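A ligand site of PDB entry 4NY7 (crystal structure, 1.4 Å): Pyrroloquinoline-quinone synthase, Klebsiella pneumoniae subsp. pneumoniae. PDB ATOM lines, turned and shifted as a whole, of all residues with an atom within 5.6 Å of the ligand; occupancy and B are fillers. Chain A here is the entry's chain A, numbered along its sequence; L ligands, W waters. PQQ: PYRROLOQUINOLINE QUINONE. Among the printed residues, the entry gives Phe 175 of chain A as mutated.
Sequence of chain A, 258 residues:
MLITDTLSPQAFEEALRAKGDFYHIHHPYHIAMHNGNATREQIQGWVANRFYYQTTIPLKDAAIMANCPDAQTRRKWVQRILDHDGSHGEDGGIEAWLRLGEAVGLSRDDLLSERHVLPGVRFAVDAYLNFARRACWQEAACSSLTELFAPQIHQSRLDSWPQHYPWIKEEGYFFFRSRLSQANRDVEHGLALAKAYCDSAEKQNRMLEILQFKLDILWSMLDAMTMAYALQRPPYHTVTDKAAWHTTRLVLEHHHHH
An oxygen (O2A) of the ligand is in hydrogen-bond range of the side-chain hydroxyl (OH) of Tyr 128. An oxygen (O7A) of the ligand lies within salt-bridge range of the guanidinium group (NH1) of Arg 157 (2.6 Å). OH of Tyr 23 is in hydrogen-bond range of O9A of the ligand (2.7 Å). NE2 of His 24 is in hydrogen-bond range of O7B of the ligand, 2.8 Å away. O9B of the ligand sits at hydrogen-bond distance from OH of Tyr 53 (2.8 Å). An oxygen (O2B) of the ligand is in salt-bridge range of the side-chain amino group of Lys 60. An oxygen (O2A) of the ligand is in salt-bridge range of the side-chain amino group (NZ) of Lys 214 (2.8 Å). OG1 of Thr 146 lies within hydrogen-bond range of O9B of the ligand, at 2.8 Å. An oxygen (O4) of the ligand sits close to a ring nitrogen (NE2) of His 84. An oxygen (O7A) of the ligand lies within salt-bridge range of the guanidinium group (NH2) of Arg 50, 3.0 Å away. An oxygen (O4) of the ligand sits close to the guanidinium group of Arg 179 (3.3 Å). An oxygen (O5) of the ligand is in hydrogen-bond range of the side-chain amide nitrogen of Gln 54, at 3.3 Å.
NZ of Lys 60 lies within hydrogen-bond range of OH of Tyr 128, 3.2 Å away. OH of Tyr 128 lies within hydrogen-bond range of NZ of Lys 214 (3.3 Å). The side-chain hydroxyl of Thr 146 is in hydrogen-bond range of the side-chain amino group of Lys 214, 2.8 Å away. The backbone carbonyl oxygen (O) of Ser 143 lies within hydrogen-bond range of the side-chain amino group (NZ) of Lys 214, at 3.0 Å. NH2 of Arg 50 sits at hydrogen-bond distance from OE1 of Gln 54 (2.7 Å). The guanidinium group (NH2) of Arg 179 lies within salt-bridge range of the side-chain carboxylate (OD2) of Asp 186, at 3.4 Å. The side-chain carboxylate (OE1) of Glu 147 lies within salt-bridge range of the guanidinium group (NH1) of Arg 80 (2.9 Å). OD2 of Asp 186 sits close to OE2 of Glu 147 (2.5 Å).
Ile 57 touches the ligand. Ser 144 touches the ligand (CA to O2A, 3.5 Å). Glu 147 touches the ligand (CG to N1, 3.8 Å). Ile 153 touches the ligand. His 154 touches the ligand. Phe 175 touches the ligand. CD1 of Leu 218 touches O9A of the ligand (3.8 Å). Hydrophobic or aromatic side chains that line the ligand: Tyr 23, His 24, Tyr 53, Ile 57, His 84, Tyr 128, Ile 153, His 154, Phe 175 and Leu 218. Of the 28 residues printed, 19 come within 4 Å of the ligand.
Water W1 lies within hydrogen-bond range of OD2 of Asp 61 (2.8 Å), O2B of the ligand (2.8 Å) and NH1 of Arg 80 (3.0 Å).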
ATOM      1  N   TYR A  23       4.204 -13.971  17.836  1.00  0.00           N
ATOM      2  CA  TYR A  23       5.199 -14.333  18.844  1.00  0.00           C
ATOM      3  C   TYR A  23       5.210 -13.341  19.992  1.00  0.00           C
ATOM      4  O   TYR A  23       4.871 -12.149  19.856  1.00  0.00           O
ATOM      5  CB  TYR A  23       6.557 -14.385  18.207  1.00  0.00           C
ATOM      6  CG  TYR A  23       7.668 -15.116  18.892  1.00  0.00           C
ATOM      7  CD1 TYR A  23       7.484 -16.433  19.309  1.00  0.00           C
ATOM      8  CD2 TYR A  23       8.916 -14.544  19.121  1.00  0.00           C
ATOM      9  CE1 TYR A  23       8.461 -17.169  19.940  1.00  0.00           C
ATOM     10  CE2 TYR A  23       9.904 -15.289  19.749  1.00  0.00           C
ATOM     11  CZ  TYR A  23       9.679 -16.570  20.143  1.00  0.00           C
ATOM     12  OH  TYR A  23      10.705 -17.239  20.755  1.00  0.00           O
ATOM     13  N   HIS A  24       5.663 -13.827  21.141  1.00  0.00           N
ATOM     14  CA  HIS A  24       5.596 -13.090  22.395  1.00  0.00           C
ATOM     15  C   HIS A  24       6.556 -11.914  22.462  1.00  0.00           C
ATOM     16  O   HIS A  24       6.508 -11.145  23.427  1.00  0.00           O
ATOM     17  CB  HIS A  24       5.815 -14.029  23.568  1.00  0.00           C
ATOM     18  CG  HIS A  24       7.132 -14.714  23.630  1.00  0.00           C
ATOM     19  ND1 HIS A  24       7.495 -15.364  24.837  1.00  0.00           N
ATOM     20  CD2 HIS A  24       8.200 -14.876  22.807  1.00  0.00           C
ATOM     21  CE1 HIS A  24       8.691 -15.896  24.710  1.00  0.00           C
ATOM     22  NE2 HIS A  24       9.150 -15.606  23.464  1.00  0.00           N
ATOM     23  N   TRP A  46      10.341 -12.531  35.912  1.00  0.00           N
ATOM     24  CA  TRP A  46      10.426 -13.173  34.603  1.00  0.00           C
ATOM     25  C   TRP A  46      11.475 -14.262  34.605  1.00  0.00           C
ATOM     26  O   TRP A  46      11.239 -15.385  34.134  1.00  0.00           O
ATOM     27  CB  TRP A  46      10.688 -12.097  33.557  1.00  0.00           C
ATOM     28  CG  TRP A  46      10.769 -12.565  32.138  1.00  0.00           C
ATOM     29  CD1 TRP A  46       9.753 -12.723  31.243  1.00  0.00           C
ATOM     30  CD2 TRP A  46      11.985 -12.935  31.457  1.00  0.00           C
ATOM     31  NE1 TRP A  46      10.255 -13.175  30.034  1.00  0.00           N
ATOM     32  CE2 TRP A  46      11.622 -13.310  30.141  1.00  0.00           C
ATOM     33  CE3 TRP A  46      13.347 -12.978  31.800  1.00  0.00           C
ATOM     34  CZ2 TRP A  46      12.565 -13.716  29.209  1.00  0.00           C
ATOM     35  CZ3 TRP A  46      14.283 -13.395  30.870  1.00  0.00           C
ATOM     36  CH2 TRP A  46      13.881 -13.766  29.572  1.00  0.00           C
ATOM     37  N   ARG A  50      10.388 -18.010  34.075  1.00  0.00           N
ATOM     38  CA  ARG A  50      10.853 -18.668  32.852  1.00  0.00           C
ATOM     39  C   ARG A  50      11.743 -19.868  33.161  1.00  0.00           C
ATOM     40  O   ARG A  50      11.846 -20.775  32.326  1.00  0.00           O
ATOM     41  CB  ARG A  50      11.557 -17.681  31.898  1.00  0.00           C
ATOM     42  CG  ARG A  50      10.692 -17.039  30.845  1.00  0.00           C
ATOM     43  CD  ARG A  50      10.246 -18.047  29.776  1.00  0.00           C
ATOM     44  NE  ARG A  50      11.439 -18.552  29.098  1.00  0.00           N
ATOM     45  CZ  ARG A  50      11.997 -17.926  28.151  1.00  0.00           C
ATOM     46  NH1 ARG A  50      11.590 -16.761  27.661  1.00  0.00           N
ATOM     47  NH2 ARG A  50      13.128 -18.492  27.578  1.00  0.00           N
ATOM     48  N   TYR A  53       9.853 -22.949  32.607  1.00  0.00           N
ATOM     49  CA  TYR A  53       9.794 -23.363  31.197  1.00  0.00           C
ATOM     50  C   TYR A  53      11.082 -24.077  30.795  1.00  0.00           C
ATOM     51  O   TYR A  53      11.060 -25.149  30.199  1.00  0.00           O
ATOM     52  CB  TYR A  53       9.516 -22.178  30.293  1.00  0.00           C
ATOM     53  CG  TYR A  53       9.334 -22.384  28.818  1.00  0.00           C
ATOM     54  CD1 TYR A  53       8.194 -22.995  28.333  1.00  0.00           C
ATOM     55  CD2 TYR A  53      10.284 -21.953  27.901  1.00  0.00           C
ATOM     56  CE1 TYR A  53       8.043 -23.161  26.984  1.00  0.00           C
ATOM     57  CE2 TYR A  53      10.116 -22.110  26.526  1.00  0.00           C
ATOM     58  CZ  TYR A  53       8.974 -22.722  26.082  1.00  0.00           C
ATOM     59  OH  TYR A  53       8.737 -22.939  24.730  1.00  0.00           O
ATOM     60  N   GLN A  54      12.214 -23.463  31.139  1.00  0.00           N
ATOM     61  CA  GLN A  54      13.516 -24.004  30.765  1.00  0.00           C
ATOM     62  C   GLN A  54      13.723 -25.398  31.335  1.00  0.00           C
ATOM     63  O   GLN A  54      14.265 -26.255  30.615  1.00  0.00           O
ATOM     64  CB  GLN A  54      14.652 -23.102  31.264  1.00  0.00           C
ATOM     65  CG  GLN A  54      14.647 -21.696  30.785  1.00  0.00           C
ATOM     66  CD  GLN A  54      14.446 -21.541  29.296  1.00  0.00           C
ATOM     67  OE1 GLN A  54      13.555 -20.791  28.892  1.00  0.00           O
ATOM     68  NE2 GLN A  54      15.267 -22.250  28.530  1.00  0.00           N
ATOM     69  N   ILE A  57      11.710 -28.031  29.258  1.00  0.00           N
ATOM     70  CA  ILE A  57      12.071 -28.364  27.885  1.00  0.00           C
ATOM     71  C   ILE A  57      12.677 -29.759  27.842  1.00  0.00           C
ATOM     72  O   ILE A  57      12.222 -30.545  27.021  1.00  0.00           O
ATOM     73  CB  ILE A  57      12.971 -27.263  27.260  1.00  0.00           C
ATOM     74  CG1 ILE A  57      12.279 -25.897  27.218  1.00  0.00           C
ATOM     75  CG2 ILE A  57      13.503 -27.717  25.891  1.00  0.00           C
ATOM     76  CD1 ILE A  57      10.938 -25.938  26.472  1.00  0.00           C
ATOM     77  N   LYS A  60       9.889 -32.397  28.160  1.00  0.00           N
ATOM     78  CA  LYS A  60       9.011 -32.558  26.982  1.00  0.00           C
ATOM     79  C   LYS A  60       9.811 -33.136  25.843  1.00  0.00           C
ATOM     80  O   LYS A  60       9.234 -33.898  25.047  1.00  0.00           O
ATOM     81  CB  LYS A  60       8.241 -31.272  26.659  1.00  0.00           C
ATOM     82  CG  LYS A  60       9.091 -30.130  26.115  1.00  0.00           C
ATOM     83  CD  LYS A  60       9.216 -30.155  24.599  1.00  0.00           C
ATOM     84  CE  LYS A  60      10.296 -29.207  24.099  1.00  0.00           C
ATOM     85  NZ  LYS A  60      10.447 -29.351  22.627  1.00  0.00           N
ATOM     86  N   ASP A  61      11.130 -32.857  25.728  1.00  0.00           N
ATOM     87  CA  ASP A  61      11.878 -33.536  24.671  1.00  0.00           C
ATOM     88  C   ASP A  61      12.019 -35.010  24.968  1.00  0.00           C
ATOM     89  O   ASP A  61      11.958 -35.834  24.035  1.00  0.00           O
ATOM     90  CB  ASP A  61      13.214 -32.810  24.525  1.00  0.00           C
ATOM     91  CG  ASP A  61      13.093 -31.509  23.763  1.00  0.00           C
ATOM     92  OD1 ASP A  61      12.227 -31.465  22.828  1.00  0.00           O
ATOM     93  OD2 ASP A  61      13.863 -30.566  24.061  1.00  0.00           O
ATOM     94  N   ARG A  80      18.907 -31.936  22.025  1.00  0.00           N
ATOM     95  CA  ARG A  80      18.195 -30.900  22.782  1.00  0.00           C
ATOM     96  C   ARG A  80      18.296 -31.129  24.290  1.00  0.00           C
ATOM     97  O   ARG A  80      18.482 -30.152  25.025  1.00  0.00           O
ATOM     98  CB  ARG A  80      16.710 -30.840  22.352  1.00  0.00           C
ATOM     99  CG  ARG A  80      16.491 -30.435  20.889  1.00  0.00           C
ATOM    100  CD  ARG A  80      15.155 -30.999  20.383  1.00  0.00           C
ATOM    101  NE  ARG A  80      14.958 -30.554  18.997  1.00  0.00           N
ATOM    102  CZ  ARG A  80      14.432 -29.437  18.603  1.00  0.00           C
ATOM    103  NH1 ARG A  80      13.959 -28.557  19.472  1.00  0.00           N
ATOM    104  NH2 ARG A  80      14.335 -29.163  17.247  1.00  0.00           N
ATOM    105  N   HIS A  84      20.313 -28.653  27.141  1.00  0.00           N
ATOM    106  CA  HIS A  84      19.790 -28.032  28.356  1.00  0.00           C
ATOM    107  C   HIS A  84      20.383 -28.625  29.618  1.00  0.00           C
ATOM    108  O   HIS A  84      20.659 -27.886  30.588  1.00  0.00           O
ATOM    109  CB  HIS A  84      18.228 -28.128  28.410  1.00  0.00           C
ATOM    110  CG  HIS A  84      17.647 -27.081  27.496  1.00  0.00           C
ATOM    111  ND1 HIS A  84      17.635 -25.763  27.835  1.00  0.00           N
ATOM    112  CD2 HIS A  84      17.120 -27.157  26.276  1.00  0.00           C
ATOM    113  CE1 HIS A  84      17.070 -25.043  26.792  1.00  0.00           C
ATOM    114  NE2 HIS A  84      16.763 -25.938  25.868  1.00  0.00           N
ATOM    115  N   TRP A  97      20.780 -20.632  32.730  1.00  0.00           N
ATOM    116  CA  TRP A  97      19.662 -19.839  33.210  1.00  0.00           C
ATOM    117  C   TRP A  97      19.852 -19.522  34.694  1.00  0.00           C
ATOM    118  O   TRP A  97      19.543 -18.416  35.154  1.00  0.00           O
ATOM    119  CB  TRP A  97      18.334 -20.559  32.895  1.00  0.00           C
ATOM    120  CG  TRP A  97      17.229 -19.570  32.956  1.00  0.00           C
ATOM    121  CD1 TRP A  97      16.552 -19.177  34.078  1.00  0.00           C
ATOM    122  CD2 TRP A  97      16.683 -18.816  31.879  1.00  0.00           C
ATOM    123  NE1 TRP A  97      15.603 -18.246  33.759  1.00  0.00           N
ATOM    124  CE2 TRP A  97      15.665 -17.992  32.410  1.00  0.00           C
ATOM    125  CE3 TRP A  97      16.937 -18.770  30.531  1.00  0.00           C
ATOM    126  CZ2 TRP A  97      14.952 -17.147  31.583  1.00  0.00           C
ATOM    127  CZ3 TRP A  97      16.227 -17.924  29.713  1.00  0.00           C
ATOM    128  CH2 TRP A  97      15.224 -17.119  30.261  1.00  0.00           C
ATOM    129  N   TYR A 128       2.244 -27.597  27.682  1.00  0.00           N
ATOM    130  CA  TYR A 128       3.212 -27.988  26.674  1.00  0.00           C
ATOM    131  C   TYR A 128       3.671 -29.430  26.886  1.00  0.00           C
ATOM    132  O   TYR A 128       3.708 -30.282  25.963  1.00  0.00           O
ATOM    133  CB  TYR A 128       4.451 -27.067  26.682  1.00  0.00           C
ATOM    134  CG  TYR A 128       5.384 -27.144  25.510  1.00  0.00           C
ATOM    135  CD1 TYR A 128       5.043 -27.742  24.310  1.00  0.00           C
ATOM    136  CD2 TYR A 128       6.670 -26.594  25.607  1.00  0.00           C
ATOM    137  CE1 TYR A 128       5.925 -27.799  23.250  1.00  0.00           C
ATOM    138  CE2 TYR A 128       7.559 -26.629  24.547  1.00  0.00           C
ATOM    139  CZ  TYR A 128       7.178 -27.232  23.354  1.00  0.00           C
ATOM    140  OH  TYR A 128       8.067 -27.268  22.294  1.00  0.00           O
ATOM    141  N   SER A 143       5.835 -28.722  17.280  1.00  0.00           N
ATOM    142  CA  SER A 143       5.415 -27.655  18.180  1.00  0.00           C
ATOM    143  C   SER A 143       6.614 -26.888  18.746  1.00  0.00           C
ATOM    144  O   SER A 143       6.461 -25.797  19.306  1.00  0.00           O
ATOM    145  CB  SER A 143       4.519 -28.176  19.299  1.00  0.00           C
ATOM    146  OG  SER A 143       5.146 -28.907  20.288  1.00  0.00           O
ATOM    147  N   SER A 144       7.825 -27.377  18.566  1.00  0.00           N
ATOM    148  CA  SER A 144       9.037 -26.621  18.894  1.00  0.00           C
ATOM    149  C   SER A 144       9.253 -25.435  17.991  1.00  0.00           C
ATOM    150  O   SER A 144      10.147 -24.648  18.293  1.00  0.00           O
ATOM    151  CB  SER A 144      10.292 -27.509  18.773  1.00  0.00           C
ATOM    152  OG  SER A 144      10.492 -27.935  17.463  1.00  0.00           O
ATOM    153  N   LEU A 145       8.539 -25.346  16.872  1.00  0.00           N
ATOM    154  CA  LEU A 145       8.920 -24.397  15.821  1.00  0.00           C
ATOM    155  C   LEU A 145       8.709 -22.941  16.130  1.00  0.00           C
ATOM    156  O   LEU A 145       9.067 -22.103  15.297  1.00  0.00           O
ATOM    157  CB  LEU A 145       8.273 -24.827  14.491  1.00  0.00           C
ATOM    158  CG  LEU A 145       9.013 -25.962  13.810  1.00  0.00           C
ATOM    159  CD1 LEU A 145       8.152 -26.434  12.615  1.00  0.00           C
ATOM    160  CD2 LEU A 145      10.395 -25.562  13.325  1.00  0.00           C
ATOM    161  N   THR A 146       8.194 -22.559  17.280  1.00  0.00           N
ATOM    162  CA  THR A 146       8.380 -21.158  17.681  1.00  0.00           C
ATOM    163  C   THR A 146       9.853 -20.777  17.831  1.00  0.00           C
ATOM    164  O   THR A 146      10.190 -19.586  17.831  1.00  0.00           O
ATOM    165  CB  THR A 146       7.601 -20.814  18.976  1.00  0.00           C
ATOM    166  OG1 THR A 146       7.936 -21.714  20.034  1.00  0.00           O
ATOM    167  CG2 THR A 146       6.106 -20.871  18.721  1.00  0.00           C
ATOM    168  N   GLU A 147      10.756 -21.757  17.944  1.00  0.00           N
ATOM    169  CA  GLU A 147      12.190 -21.515  17.866  1.00  0.00           C
ATOM    170  C   GLU A 147      12.579 -20.790  16.608  1.00  0.00           C
ATOM    171  O   GLU A 147      13.625 -20.154  16.551  1.00  0.00           O
ATOM    172  CB  GLU A 147      12.955 -22.855  17.975  1.00  0.00           C
ATOM    173  CG  GLU A 147      13.051 -23.425  19.390  1.00  0.00           C
ATOM    174  CD  GLU A 147      13.875 -24.711  19.324  1.00  0.00           C
ATOM    175  OE1 GLU A 147      13.466 -25.734  18.829  1.00  0.00           O
ATOM    176  OE2 GLU A 147      15.089 -24.556  19.821  1.00  0.00           O
ATOM    177  N   ALA A 150      12.939 -17.317  17.835  1.00  0.00           N
ATOM    178  CA  ALA A 150      13.667 -17.096  19.076  1.00  0.00           C
ATOM    179  C   ALA A 150      14.998 -16.389  18.890  1.00  0.00           C
ATOM    180  O   ALA A 150      15.300 -15.502  19.733  1.00  0.00           O
ATOM    181  CB  ALA A 150      13.858 -18.467  19.782  1.00  0.00           C
ATOM    182  N   ILE A 153      14.407 -12.695  19.283  1.00  0.00           N
ATOM    183  CA  ILE A 153      14.117 -12.180  20.613  1.00  0.00           C
ATOM    184  C   ILE A 153      15.347 -12.248  21.503  1.00  0.00           C
ATOM    185  O   ILE A 153      15.619 -11.312  22.281  1.00  0.00           O
ATOM    186  CB  ILE A 153      12.884 -12.839  21.259  1.00  0.00           C
ATOM    187  CG1 ILE A 153      12.304 -11.950  22.365  1.00  0.00           C
ATOM    188  CG2 ILE A 153      13.122 -14.258  21.761  1.00  0.00           C
ATOM    189  CD1 ILE A 153      10.914 -12.330  22.821  1.00  0.00           C
ATOM    190  N   HIS A 154      16.132 -13.297  21.446  1.00  0.00           N
ATOM    191  CA  HIS A 154      17.376 -13.369  22.201  1.00  0.00           C
ATOM    192  C   HIS A 154      18.269 -12.185  21.792  1.00  0.00           C
ATOM    193  O   HIS A 154      18.788 -11.545  22.680  1.00  0.00           O
ATOM    194  CB  HIS A 154      18.126 -14.680  22.007  1.00  0.00           C
ATOM    195  CG  HIS A 154      17.425 -15.874  22.540  1.00  0.00           C
ATOM    196  ND1 HIS A 154      17.077 -15.991  23.836  1.00  0.00           N
ATOM    197  CD2 HIS A 154      16.987 -17.018  21.927  1.00  0.00           C
ATOM    198  CE1 HIS A 154      16.466 -17.122  24.045  1.00  0.00           C
ATOM    199  NE2 HIS A 154      16.407 -17.785  22.827  1.00  0.00           N
ATOM    200  N   ARG A 157      17.315  -8.817  23.370  1.00  0.00           N
ATOM    201  CA  ARG A 157      17.749  -8.627  24.763  1.00  0.00           C
ATOM    202  C   ARG A 157      19.237  -8.293  24.858  1.00  0.00           C
ATOM    203  O   ARG A 157      19.659  -7.429  25.615  1.00  0.00           O
ATOM    204  CB  ARG A 157      17.481  -9.879  25.615  1.00  0.00           C
ATOM    205  CG  ARG A 157      16.018 -10.320  25.524  1.00  0.00           C
ATOM    206  CD  ARG A 157      15.763 -11.684  26.169  1.00  0.00           C
ATOM    207  NE  ARG A 157      14.401 -12.212  26.016  1.00  0.00           N
ATOM    208  CZ  ARG A 157      14.050 -13.393  25.650  1.00  0.00           C
ATOM    209  NH1 ARG A 157      14.847 -14.373  25.347  1.00  0.00           N
ATOM    210  NH2 ARG A 157      12.679 -13.643  25.583  1.00  0.00           N
ATOM    211  N   PHE A 175      23.285 -17.327  28.228  1.00  0.00           N
ATOM    212  CA  PHE A 175      22.250 -18.215  27.678  1.00  0.00           C
ATOM    213  C   PHE A 175      21.708 -17.665  26.385  1.00  0.00           C
ATOM    214  O   PHE A 175      21.568 -18.405  25.377  1.00  0.00           O
ATOM    215  CB  PHE A 175      21.129 -18.409  28.713  1.00  0.00           C
ATOM    216  CG  PHE A 175      20.050 -19.342  28.172  1.00  0.00           C
ATOM    217  CD1 PHE A 175      20.218 -20.703  28.169  1.00  0.00           C
ATOM    218  CD2 PHE A 175      18.878 -18.826  27.651  1.00  0.00           C
ATOM    219  CE1 PHE A 175      19.253 -21.551  27.636  1.00  0.00           C
ATOM    220  CE2 PHE A 175      17.917 -19.675  27.138  1.00  0.00           C
ATOM    221  CZ  PHE A 175      18.083 -21.035  27.124  1.00  0.00           C
ATOM    222  N   PHE A 176      21.356 -16.396  26.334  1.00  0.00           N
ATOM    223  CA  PHE A 176      20.765 -15.825  25.122  1.00  0.00           C
ATOM    224  C   PHE A 176      21.710 -15.971  23.957  1.00  0.00           C
ATOM    225  O   PHE A 176      21.285 -16.311  22.868  1.00  0.00           O
ATOM    226  CB  PHE A 176      20.400 -14.354  25.289  1.00  0.00           C
ATOM    227  CG  PHE A 176      19.472 -14.033  26.442  1.00  0.00           C
ATOM    228  CD1 PHE A 176      18.469 -14.869  26.887  1.00  0.00           C
ATOM    229  CD2 PHE A 176      19.635 -12.825  27.111  1.00  0.00           C
ATOM    230  CE1 PHE A 176      17.675 -14.520  27.961  1.00  0.00           C
ATOM    231  CE2 PHE A 176      18.848 -12.455  28.184  1.00  0.00           C
ATOM    232  CZ  PHE A 176      17.858 -13.319  28.626  1.00  0.00           C
ATOM    233  N   ARG A 179      21.791 -19.563  22.495  1.00  0.00           N
ATOM    234  CA  ARG A 179      20.608 -19.968  21.734  1.00  0.00           C
ATOM    235  C   ARG A 179      20.598 -19.408  20.332  1.00  0.00           C
ATOM    236  O   ARG A 179      19.871 -19.965  19.486  1.00  0.00           O
ATOM    237  CB  ARG A 179      19.316 -19.590  22.502  1.00  0.00           C
ATOM    238  CG  ARG A 179      19.093 -20.267  23.850  1.00  0.00           C
ATOM    239  CD  ARG A 179      19.214 -21.791  23.763  1.00  0.00           C
ATOM    240  NE  ARG A 179      18.082 -22.271  23.001  1.00  0.00           N
ATOM    241  CZ  ARG A 179      17.778 -23.478  22.697  1.00  0.00           C
ATOM    242  NH1 ARG A 179      18.636 -24.473  23.086  1.00  0.00           N
ATOM    243  NH2 ARG A 179      16.735 -23.849  22.041  1.00  0.00           N
ATOM    244  N   ASP A 186      18.253 -26.366  15.759  1.00  0.00           N
ATOM    245  CA  ASP A 186      17.024 -27.055  16.098  1.00  0.00           C
ATOM    246  C   ASP A 186      16.012 -26.983  14.969  1.00  0.00           C
ATOM    247  O   ASP A 186      15.465 -28.027  14.594  1.00  0.00           O
ATOM    248  CB  ASP A 186      16.449 -26.464  17.394  1.00  0.00           C
ATOM    249  CG  ASP A 186      17.117 -26.867  18.694  1.00  0.00           C
ATOM    250  OD1 ASP A 186      18.087 -27.701  18.621  1.00  0.00           O
ATOM    251  OD2 ASP A 186      16.765 -26.392  19.791  1.00  0.00           O
ATOM    252  N   LYS A 214       1.037 -23.367  20.815  1.00  0.00           N
ATOM    253  CA  LYS A 214       2.330 -23.042  21.359  1.00  0.00           C
ATOM    254  C   LYS A 214       2.527 -21.564  21.615  1.00  0.00           C
ATOM    255  O   LYS A 214       2.988 -21.149  22.677  1.00  0.00           O
ATOM    256  CB  LYS A 214       3.434 -23.550  20.444  1.00  0.00           C
ATOM    257  CG  LYS A 214       4.826 -23.242  20.957  1.00  0.00           C
ATOM    258  CD  LYS A 214       5.236 -24.058  22.184  1.00  0.00           C
ATOM    259  CE  LYS A 214       6.668 -23.791  22.566  1.00  0.00           C
ATOM    260  NZ  LYS A 214       7.645 -24.118  21.495  1.00  0.00           N
ATOM    261  N   LEU A 218       3.122 -19.243  25.318  1.00  0.00           N
ATOM    262  CA  LEU A 218       4.094 -18.172  25.575  1.00  0.00           C
ATOM    263  C   LEU A 218       3.414 -16.891  26.041  1.00  0.00           C
ATOM    264  O   LEU A 218       3.804 -16.249  27.007  1.00  0.00           O
ATOM    265  CB  LEU A 218       4.948 -17.913  24.330  1.00  0.00           C
ATOM    266  CG  LEU A 218       5.799 -19.102  23.851  1.00  0.00           C
ATOM    267  CD1 LEU A 218       6.572 -18.722  22.592  1.00  0.00           C
ATOM    268  CD2 LEU A 218       6.753 -19.613  24.917  1.00  0.00           C
HETATM  269  N1  PQQ L   1      11.473 -23.351  22.798  1.00  0.00           N
HETATM  270  C2  PQQ L   1      11.980 -24.592  22.919  1.00  0.00           C
HETATM  271  C2X PQQ L   1      11.224 -25.608  22.444  1.00  0.00           C
HETATM  272  O2A PQQ L   1       9.963 -25.564  22.142  1.00  0.00           O
HETATM  273  O2B PQQ L   1      11.594 -26.830  22.359  1.00  0.00           O
HETATM  274  C3  PQQ L   1      13.264 -24.640  23.431  1.00  0.00           C
HETATM  275  C3A PQQ L   1      13.465 -23.235  23.758  1.00  0.00           C
HETATM  276  C1A PQQ L   1      12.406 -22.466  23.348  1.00  0.00           C
HETATM  277  C4  PQQ L   1      14.436 -22.666  24.543  1.00  0.00           C
HETATM  278  O4  PQQ L   1      15.510 -23.364  25.022  1.00  0.00           O
HETATM  279  C5  PQQ L   1      14.431 -21.245  24.881  1.00  0.00           C
HETATM  280  O5  PQQ L   1      15.335 -20.615  25.680  1.00  0.00           O
HETATM  281  C6A PQQ L   1      13.321 -20.457  24.288  1.00  0.00           C
HETATM  282  N6  PQQ L   1      13.438 -19.171  24.579  1.00  0.00           N
HETATM  283  C7  PQQ L   1      12.479 -18.398  24.108  1.00  0.00           C
HETATM  284  C7X PQQ L   1      12.587 -17.038  24.556  1.00  0.00           C
HETATM  285  O7A PQQ L   1      13.587 -16.627  25.333  1.00  0.00           O
HETATM  286  O7B PQQ L   1      11.768 -16.109  24.169  1.00  0.00           O
HETATM  287  C8  PQQ L   1      11.389 -18.803  23.400  1.00  0.00           C
HETATM  288  C9  PQQ L   1      11.303 -20.176  23.101  1.00  0.00           C
HETATM  289  C9X PQQ L   1      10.247 -20.508  22.152  1.00  0.00           C
HETATM  290  O9A PQQ L   1       9.870 -19.806  21.162  1.00  0.00           O
HETATM  291  O9B PQQ L   1       9.499 -21.618  22.409  1.00  0.00           O
HETATM  292  C9A PQQ L   1      12.301 -21.133  23.492  1.00  0.00           C
HETATM  293  O   HOH W   1      13.955 -28.342  22.415  1.00  0.00           O
